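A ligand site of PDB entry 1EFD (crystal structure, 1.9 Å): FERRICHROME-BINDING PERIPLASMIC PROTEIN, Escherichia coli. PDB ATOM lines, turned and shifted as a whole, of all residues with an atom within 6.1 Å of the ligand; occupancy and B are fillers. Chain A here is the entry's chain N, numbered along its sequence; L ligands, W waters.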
ATOM      1  N   GLU A  12      -0.470 -38.337  16.204  1.00  0.00           N
ATOM      2  CA  GLU A  12      -0.397 -36.979  15.675  1.00  0.00           C
ATOM      3  C   GLU A  12      -1.805 -36.419  15.763  1.00  0.00           C
ATOM      4  O   GLU A  12      -2.772 -37.182  15.789  1.00  0.00           O
ATOM      5  CB  GLU A  12       0.120 -37.017  14.224  1.00  0.00           C
ATOM      6  CG  GLU A  12       0.945 -35.793  13.834  1.00  0.00           C
ATOM      7  CD  GLU A  12       0.101 -34.549  13.691  1.00  0.00           C
ATOM      8  OE1 GLU A  12      -0.730 -34.501  12.763  1.00  0.00           O
ATOM      9  OE2 GLU A  12       0.250 -33.637  14.532  1.00  0.00           O
ATOM     10  N   TRP A  13      -1.935 -35.090  15.799  1.00  0.00           N
ATOM     11  CA  TRP A  13      -3.254 -34.473  15.945  1.00  0.00           C
ATOM     12  C   TRP A  13      -4.179 -34.477  14.745  1.00  0.00           C
ATOM     13  O   TRP A  13      -5.394 -34.287  14.899  1.00  0.00           O
ATOM     14  CB  TRP A  13      -3.093 -33.037  16.473  1.00  0.00           C
ATOM     15  CG  TRP A  13      -2.308 -32.970  17.762  1.00  0.00           C
ATOM     16  CD1 TRP A  13      -2.183 -33.948  18.702  1.00  0.00           C
ATOM     17  CD2 TRP A  13      -1.511 -31.868  18.223  1.00  0.00           C
ATOM     18  NE1 TRP A  13      -1.352 -33.539  19.722  1.00  0.00           N
ATOM     19  CE2 TRP A  13      -0.922 -32.262  19.452  1.00  0.00           C
ATOM     20  CE3 TRP A  13      -1.236 -30.582  17.726  1.00  0.00           C
ATOM     21  CZ2 TRP A  13      -0.074 -31.418  20.182  1.00  0.00           C
ATOM     22  CZ3 TRP A  13      -0.395 -29.743  18.446  1.00  0.00           C
ATOM     23  CH2 TRP A  13       0.183 -30.164  19.669  1.00  0.00           C
ATOM     24  N   ASN A  34      -0.154 -30.152  24.941  1.00  0.00           N
ATOM     25  CA  ASN A  34      -0.113 -29.122  23.909  1.00  0.00           C
ATOM     26  C   ASN A  34      -1.301 -29.181  22.982  1.00  0.00           C
ATOM     27  O   ASN A  34      -1.641 -28.191  22.340  1.00  0.00           O
ATOM     28  CB  ASN A  34       1.188 -29.197  23.130  1.00  0.00           C
ATOM     29  CG  ASN A  34       2.365 -28.649  23.927  1.00  0.00           C
ATOM     30  OD1 ASN A  34       2.285 -27.536  24.453  1.00  0.00           O
ATOM     31  ND2 ASN A  34       3.447 -29.407  23.997  1.00  0.00           N
ATOM     32  N   TRP A  38      -2.995 -25.822  21.291  1.00  0.00           N
ATOM     33  CA  TRP A  38      -3.068 -25.575  19.845  1.00  0.00           C
ATOM     34  C   TRP A  38      -4.333 -26.004  19.093  1.00  0.00           C
ATOM     35  O   TRP A  38      -4.779 -25.311  18.177  1.00  0.00           O
ATOM     36  CB  TRP A  38      -1.853 -26.205  19.150  1.00  0.00           C
ATOM     37  CG  TRP A  38      -0.560 -25.635  19.576  1.00  0.00           C
ATOM     38  CD1 TRP A  38       0.202 -26.007  20.647  1.00  0.00           C
ATOM     39  CD2 TRP A  38       0.155 -24.575  18.919  1.00  0.00           C
ATOM     40  NE1 TRP A  38       1.354 -25.252  20.697  1.00  0.00           N
ATOM     41  CE2 TRP A  38       1.351 -24.371  19.651  1.00  0.00           C
ATOM     42  CE3 TRP A  38      -0.093 -23.784  17.789  1.00  0.00           C
ATOM     43  CZ2 TRP A  38       2.293 -23.401  19.280  1.00  0.00           C
ATOM     44  CZ3 TRP A  38       0.843 -22.827  17.420  1.00  0.00           C
ATOM     45  CH2 TRP A  38       2.023 -22.644  18.165  1.00  0.00           C
ATOM     46  N   ARG A  54       4.587 -36.190  19.967  1.00  0.00           N
ATOM     47  CA  ARG A  54       4.310 -36.761  18.647  1.00  0.00           C
ATOM     48  C   ARG A  54       5.622 -37.087  17.958  1.00  0.00           C
ATOM     49  O   ARG A  54       5.693 -38.000  17.145  1.00  0.00           O
ATOM     50  CB  ARG A  54       3.508 -35.770  17.797  1.00  0.00           C
ATOM     51  CG  ARG A  54       2.191 -35.371  18.413  1.00  0.00           C
ATOM     52  CD  ARG A  54       2.131 -33.865  18.587  1.00  0.00           C
ATOM     53  NE  ARG A  54       1.877 -33.195  17.329  1.00  0.00           N
ATOM     54  CZ  ARG A  54       2.311 -31.976  17.012  1.00  0.00           C
ATOM     55  NH1 ARG A  54       3.052 -31.268  17.860  1.00  0.00           N
ATOM     56  NH2 ARG A  54       1.983 -31.463  15.842  1.00  0.00           N
ATOM     57  N   THR A  55       6.674 -36.341  18.305  1.00  0.00           N
ATOM     58  CA  THR A  55       7.992 -36.536  17.709  1.00  0.00           C
ATOM     59  C   THR A  55       8.870 -37.545  18.434  1.00  0.00           C
ATOM     60  O   THR A  55       9.836 -38.056  17.864  1.00  0.00           O
ATOM     61  CB  THR A  55       8.759 -35.203  17.638  1.00  0.00           C
ATOM     62  OG1 THR A  55       8.720 -34.563  18.921  1.00  0.00           O
ATOM     63  CG2 THR A  55       8.123 -34.279  16.598  1.00  0.00           C
ATOM     64  N   TYR A  76       5.611 -37.017   9.022  1.00  0.00           N
ATOM     65  CA  TYR A  76       5.828 -36.346  10.301  1.00  0.00           C
ATOM     66  C   TYR A  76       6.087 -37.354  11.427  1.00  0.00           C
ATOM     67  O   TYR A  76       5.479 -38.428  11.477  1.00  0.00           O
ATOM     68  CB  TYR A  76       4.595 -35.509  10.674  1.00  0.00           C
ATOM     69  CG  TYR A  76       4.737 -34.747  11.966  1.00  0.00           C
ATOM     70  CD1 TYR A  76       5.143 -33.419  11.974  1.00  0.00           C
ATOM     71  CD2 TYR A  76       4.519 -35.369  13.201  1.00  0.00           C
ATOM     72  CE1 TYR A  76       5.318 -32.720  13.173  1.00  0.00           C
ATOM     73  CE2 TYR A  76       4.692 -34.695  14.396  1.00  0.00           C
ATOM     74  CZ  TYR A  76       5.090 -33.366  14.380  1.00  0.00           C
ATOM     75  OH  TYR A  76       5.231 -32.690  15.578  1.00  0.00           O
ATOM     76  N   THR A 151      -0.059 -16.434  13.018  1.00  0.00           N
ATOM     77  CA  THR A 151       0.093 -16.914  14.384  1.00  0.00           C
ATOM     78  C   THR A 151       1.551 -16.643  14.745  1.00  0.00           C
ATOM     79  O   THR A 151       2.454 -16.848  13.932  1.00  0.00           O
ATOM     80  CB  THR A 151      -0.260 -18.426  14.531  1.00  0.00           C
ATOM     81  OG1 THR A 151      -0.451 -18.724  15.931  1.00  0.00           O
ATOM     82  CG2 THR A 151       0.843 -19.315  13.985  1.00  0.00           C
ATOM     83  N   ILE A 153       5.031 -17.330  16.379  1.00  0.00           N
ATOM     84  CA  ILE A 153       5.863 -18.441  16.835  1.00  0.00           C
ATOM     85  C   ILE A 153       6.699 -17.923  18.018  1.00  0.00           C
ATOM     86  O   ILE A 153       6.756 -18.532  19.078  1.00  0.00           O
ATOM     87  CB  ILE A 153       6.791 -18.937  15.713  1.00  0.00           C
ATOM     88  CG1 ILE A 153       5.954 -19.467  14.564  1.00  0.00           C
ATOM     89  CG2 ILE A 153       7.703 -20.032  16.246  1.00  0.00           C
ATOM     90  CD1 ILE A 153       4.907 -20.494  14.990  1.00  0.00           C
ATOM     91  N   LEU A 159       4.003 -16.847  11.592  1.00  0.00           N
ATOM     92  CA  LEU A 159       3.648 -17.797  10.555  1.00  0.00           C
ATOM     93  C   LEU A 159       2.515 -17.150   9.794  1.00  0.00           C
ATOM     94  O   LEU A 159       1.676 -16.454  10.377  1.00  0.00           O
ATOM     95  CB  LEU A 159       3.124 -19.127  11.114  1.00  0.00           C
ATOM     96  CG  LEU A 159       4.056 -20.289  11.426  1.00  0.00           C
ATOM     97  CD1 LEU A 159       3.195 -21.535  11.580  1.00  0.00           C
ATOM     98  CD2 LEU A 159       5.072 -20.484  10.308  1.00  0.00           C
ATOM     99  N   ASN A 185       5.238 -24.050   2.765  1.00  0.00           N
ATOM    100  CA  ASN A 185       5.772 -25.395   2.781  1.00  0.00           C
ATOM    101  C   ASN A 185       4.602 -26.326   2.446  1.00  0.00           C
ATOM    102  O   ASN A 185       3.498 -25.869   2.111  1.00  0.00           O
ATOM    103  CB  ASN A 185       6.386 -25.759   4.145  1.00  0.00           C
ATOM    104  CG  ASN A 185       5.437 -25.529   5.311  1.00  0.00           C
ATOM    105  OD1 ASN A 185       4.225 -25.443   5.144  1.00  0.00           O
ATOM    106  ND2 ASN A 185       5.998 -25.427   6.510  1.00  0.00           N
ATOM    107  N   TRP A 187       2.783 -27.932   4.310  1.00  0.00           N
ATOM    108  CA  TRP A 187       1.690 -27.728   5.260  1.00  0.00           C
ATOM    109  C   TRP A 187       0.877 -26.460   5.064  1.00  0.00           C
ATOM    110  O   TRP A 187      -0.109 -26.252   5.762  1.00  0.00           O
ATOM    111  CB  TRP A 187       2.241 -27.807   6.684  1.00  0.00           C
ATOM    112  CG  TRP A 187       2.947 -29.096   6.946  1.00  0.00           C
ATOM    113  CD1 TRP A 187       4.239 -29.415   6.631  1.00  0.00           C
ATOM    114  CD2 TRP A 187       2.349 -30.294   7.475  1.00  0.00           C
ATOM    115  NE1 TRP A 187       4.484 -30.737   6.915  1.00  0.00           N
ATOM    116  CE2 TRP A 187       3.350 -31.300   7.433  1.00  0.00           C
ATOM    117  CE3 TRP A 187       1.082 -30.612   7.962  1.00  0.00           C
ATOM    118  CZ2 TRP A 187       3.109 -32.604   7.879  1.00  0.00           C
ATOM    119  CZ3 TRP A 187       0.842 -31.916   8.408  1.00  0.00           C
ATOM    120  CH2 TRP A 187       1.856 -32.897   8.363  1.00  0.00           C
ATOM    121  N   SER A 189       2.133 -23.148   5.176  1.00  0.00           N
ATOM    122  CA  SER A 189       2.591 -21.966   5.889  1.00  0.00           C
ATOM    123  C   SER A 189       4.073 -21.686   5.725  1.00  0.00           C
ATOM    124  O   SER A 189       4.824 -22.476   5.168  1.00  0.00           O
ATOM    125  CB  SER A 189       2.271 -22.109   7.378  1.00  0.00           C
ATOM    126  OG  SER A 189       2.855 -23.284   7.933  1.00  0.00           O
ATOM    127  N   ALA A 191       7.233 -18.991   7.852  1.00  0.00           N
ATOM    128  CA  ALA A 191       7.520 -18.035   8.903  1.00  0.00           C
ATOM    129  C   ALA A 191       8.226 -16.815   8.308  1.00  0.00           C
ATOM    130  O   ALA A 191       9.156 -16.951   7.515  1.00  0.00           O
ATOM    131  CB  ALA A 191       8.406 -18.675   9.977  1.00  0.00           C
ATOM    132  N   TRP A 243      -6.462 -25.450  15.024  1.00  0.00           N
ATOM    133  CA  TRP A 243      -5.352 -26.243  14.497  1.00  0.00           C
ATOM    134  C   TRP A 243      -5.265 -26.033  12.991  1.00  0.00           C
ATOM    135  O   TRP A 243      -6.226 -26.274  12.268  1.00  0.00           O
ATOM    136  CB  TRP A 243      -5.542 -27.732  14.801  1.00  0.00           C
ATOM    137  CG  TRP A 243      -4.329 -28.566  14.487  1.00  0.00           C
ATOM    138  CD1 TRP A 243      -4.297 -29.787  13.872  1.00  0.00           C
ATOM    139  CD2 TRP A 243      -2.967 -28.244  14.792  1.00  0.00           C
ATOM    140  NE1 TRP A 243      -3.007 -30.251  13.785  1.00  0.00           N
ATOM    141  CE2 TRP A 243      -2.164 -29.322  14.344  1.00  0.00           C
ATOM    142  CE3 TRP A 243      -2.337 -27.153  15.409  1.00  0.00           C
ATOM    143  CZ2 TRP A 243      -0.781 -29.342  14.489  1.00  0.00           C
ATOM    144  CZ3 TRP A 243      -0.954 -27.173  15.554  1.00  0.00           C
ATOM    145  CH2 TRP A 243      -0.191 -28.254  15.098  1.00  0.00           C
ATOM    146  N   PHE A 244      -4.110 -25.580  12.517  1.00  0.00           N
ATOM    147  CA  PHE A 244      -3.943 -25.297  11.095  1.00  0.00           C
ATOM    148  C   PHE A 244      -3.595 -26.503  10.241  1.00  0.00           C
ATOM    149  O   PHE A 244      -3.642 -26.417   9.013  1.00  0.00           O
ATOM    150  CB  PHE A 244      -2.868 -24.247  10.881  1.00  0.00           C
ATOM    151  CG  PHE A 244      -2.495 -23.488  12.120  1.00  0.00           C
ATOM    152  CD1 PHE A 244      -1.381 -23.853  12.856  1.00  0.00           C
ATOM    153  CD2 PHE A 244      -3.249 -22.409  12.525  1.00  0.00           C
ATOM    154  CE1 PHE A 244      -1.019 -23.143  13.988  1.00  0.00           C
ATOM    155  CE2 PHE A 244      -2.903 -21.684  13.651  1.00  0.00           C
ATOM    156  CZ  PHE A 244      -1.789 -22.050  14.387  1.00  0.00           C
ATOM    157  N   TYR A 245      -3.246 -27.613  10.873  1.00  0.00           N
ATOM    158  CA  TYR A 245      -2.846 -28.805  10.143  1.00  0.00           C
ATOM    159  C   TYR A 245      -3.747 -30.000  10.392  1.00  0.00           C
ATOM    160  O   TYR A 245      -3.297 -31.146  10.359  1.00  0.00           O
ATOM    161  CB  TYR A 245      -1.398 -29.134  10.521  1.00  0.00           C
ATOM    162  CG  TYR A 245      -0.509 -27.913  10.464  1.00  0.00           C
ATOM    163  CD1 TYR A 245       0.179 -27.468  11.591  1.00  0.00           C
ATOM    164  CD2 TYR A 245      -0.380 -27.172   9.273  1.00  0.00           C
ATOM    165  CE1 TYR A 245       0.985 -26.323  11.546  1.00  0.00           C
ATOM    166  CE2 TYR A 245       0.419 -26.032   9.217  1.00  0.00           C
ATOM    167  CZ  TYR A 245       1.100 -25.606  10.358  1.00  0.00           C
ATOM    168  OH  TYR A 245       1.912 -24.498  10.292  1.00  0.00           O
HETATM  169  C1  LIG L   1       7.136 -23.701  14.921  1.00  0.00           C
HETATM  170  C2  LIG L   1      12.904 -25.800  13.038  1.00  0.00           C
HETATM  171  C3  LIG L   1       3.279 -27.026  14.210  1.00  0.00           C
HETATM  172  C4  LIG L   1       5.867 -24.800  11.932  1.00  0.00           C
HETATM  173  C5  LIG L   1      10.575 -23.972  13.731  1.00  0.00           C
HETATM  174  C6  LIG L   1       3.010 -29.972  12.382  1.00  0.00           C
HETATM  175  C7  LIG L   1       8.181 -26.889  11.230  1.00  0.00           C
HETATM  176  C8  LIG L   1      11.531 -28.332  11.479  1.00  0.00           C
HETATM  177  C9  LIG L   1       6.882 -29.754  15.782  1.00  0.00           C
HETATM  178  C10 LIG L   1       5.803 -23.886  14.206  1.00  0.00           C
HETATM  179  C11 LIG L   1      12.936 -24.287  13.220  1.00  0.00           C
HETATM  180  C12 LIG L   1       5.864 -26.008  10.989  1.00  0.00           C
HETATM  181  C13 LIG L   1       9.547 -23.575  14.740  1.00  0.00           C
HETATM  182  C14 LIG L   1       9.102 -28.007  11.750  1.00  0.00           C
HETATM  183  C15 LIG L   1      12.930 -27.692  11.487  1.00  0.00           C
HETATM  184  C16 LIG L   1       4.655 -24.124  15.196  1.00  0.00           C
HETATM  185  C17 LIG L   1       4.453 -26.643  10.977  1.00  0.00           C
HETATM  186  C18 LIG L   1       8.738 -28.408  13.190  1.00  0.00           C
HETATM  187  C19 LIG L   1       3.284 -24.139  14.566  1.00  0.00           C
HETATM  188  C20 LIG L   1       4.223 -27.767   9.929  1.00  0.00           C
HETATM  189  C21 LIG L   1       9.046 -27.368  14.277  1.00  0.00           C
HETATM  190  C22 LIG L   1       2.309 -25.098  15.233  1.00  0.00           C
HETATM  191  C23 LIG L   1       4.443 -29.237  10.384  1.00  0.00           C
HETATM  192  C24 LIG L   1       8.607 -27.842  15.667  1.00  0.00           C
HETATM  193  C25 LIG L   1       1.897 -30.713  11.608  1.00  0.00           C
HETATM  194  C26 LIG L   1       4.535 -28.605  14.523  1.00  0.00           C
HETATM  195  C27 LIG L   1       7.865 -30.876  16.168  1.00  0.00           C
HETATM  196 GA1  LIG L   1       2.275 -26.939  17.822  1.00  0.00          GA
HETATM  197  N1  LIG L   1       5.859 -25.014  13.255  1.00  0.00           N
HETATM  198  N2  LIG L   1      11.864 -23.837  14.100  1.00  0.00           N
HETATM  199  N3  LIG L   1       6.847 -27.024  11.432  1.00  0.00           N
HETATM  200  N4  LIG L   1      10.488 -27.528  11.712  1.00  0.00           N
HETATM  201  N5  LIG L   1       2.861 -26.462  15.407  1.00  0.00           N
HETATM  202  N6  LIG L   1       4.135 -29.512  11.794  1.00  0.00           N
HETATM  203  N7  LIG L   1       8.220 -23.781  14.191  1.00  0.00           N
HETATM  204  N8  LIG L   1       7.267 -28.461  15.636  1.00  0.00           N
HETATM  205  N9  LIG L   1      12.944 -26.259  11.771  1.00  0.00           N
HETATM  206  O1  LIG L   1       7.176 -23.512  16.129  1.00  0.00           O
HETATM  207  O2  LIG L   1      12.815 -26.518  14.031  1.00  0.00           O
HETATM  208  O3  LIG L   1       3.545 -28.369  16.376  1.00  0.00           O
HETATM  209  O4  LIG L   1       5.853 -23.671  11.454  1.00  0.00           O
HETATM  210  O5  LIG L   1      10.225 -24.454  12.647  1.00  0.00           O
HETATM  211  O6  LIG L   1       3.041 -30.098  13.670  1.00  0.00           O
HETATM  212  O7  LIG L   1       8.665 -25.903  10.657  1.00  0.00           O
HETATM  213  O8  LIG L   1       5.623 -30.016  15.664  1.00  0.00           O
HETATM  214  O9  LIG L   1       3.015 -27.222  16.518  1.00  0.00           O
HETATM  215  O10 LIG L   1       5.210 -29.243  12.630  1.00  0.00           O
HETATM  216  O11 LIG L   1       6.288 -27.531  15.395  1.00  0.00           O
HETATM  217  O12 LIG L   1      11.409 -29.542  11.271  1.00  0.00           O
HETATM  218  O   HOH W   1       6.572 -27.843  18.851  1.00  0.00           O
HETATM  219  O   HOH W   2       5.346 -23.489   8.638  1.00  0.00           O
HETATM  220  O   HOH W   3       9.303 -22.893  10.510  1.00  0.00           O
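OH of Tyr 76 is in hydrogen-bond range of O8 of the ligand. An oxygen (O6) of the ligand lies within hydrogen-bond range of the guanidinium group of Arg 54 (2.8 Å).
OH of Tyr 76 sits close to NH1 of Arg 54 (3.5 Å). OE2 of Glu 12 lies within salt-bridge range of NH2 of Arg 54. OH of Tyr 245 lies within hydrogen-bond range of OG of Ser 189. The backbone carbonyl oxygen (O) of Thr 151 lies within hydrogen-bond range of the backbone NH (N) of Leu 159 (2.8 Å). The backbone NH (N) of Trp 187 sits at hydrogen-bond distance from the side-chain amide oxygen (OD1) of Asn 185 (3.0 Å).
Merely in contact with the ligand: Trp 13, Trp 38, Thr 55, Ile 153, Leu 159, Trp 187, Trp 243 and Tyr 245. Hydrophobic or aromatic side chains that line the ligand: Trp 13, Trp 38, Tyr 76, Ile 153, Leu 159, Trp 187, Trp 243 and Tyr 245. Within 4 Å of the ligand: Trp 13, Trp 38, Arg 54, Thr 55, Tyr 76, Ile 153, Leu 159, Trp 187, Trp 243 and Tyr 245. The nearest printed residue that does not touch the ligand is Phe 244 (4.1 Å).
Water W2 lies within hydrogen-bond range of OG of Ser 189 (2.6 Å), O4 of the ligand (2.9 Å) and ND2 of Asn 185 (3.0 Å).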
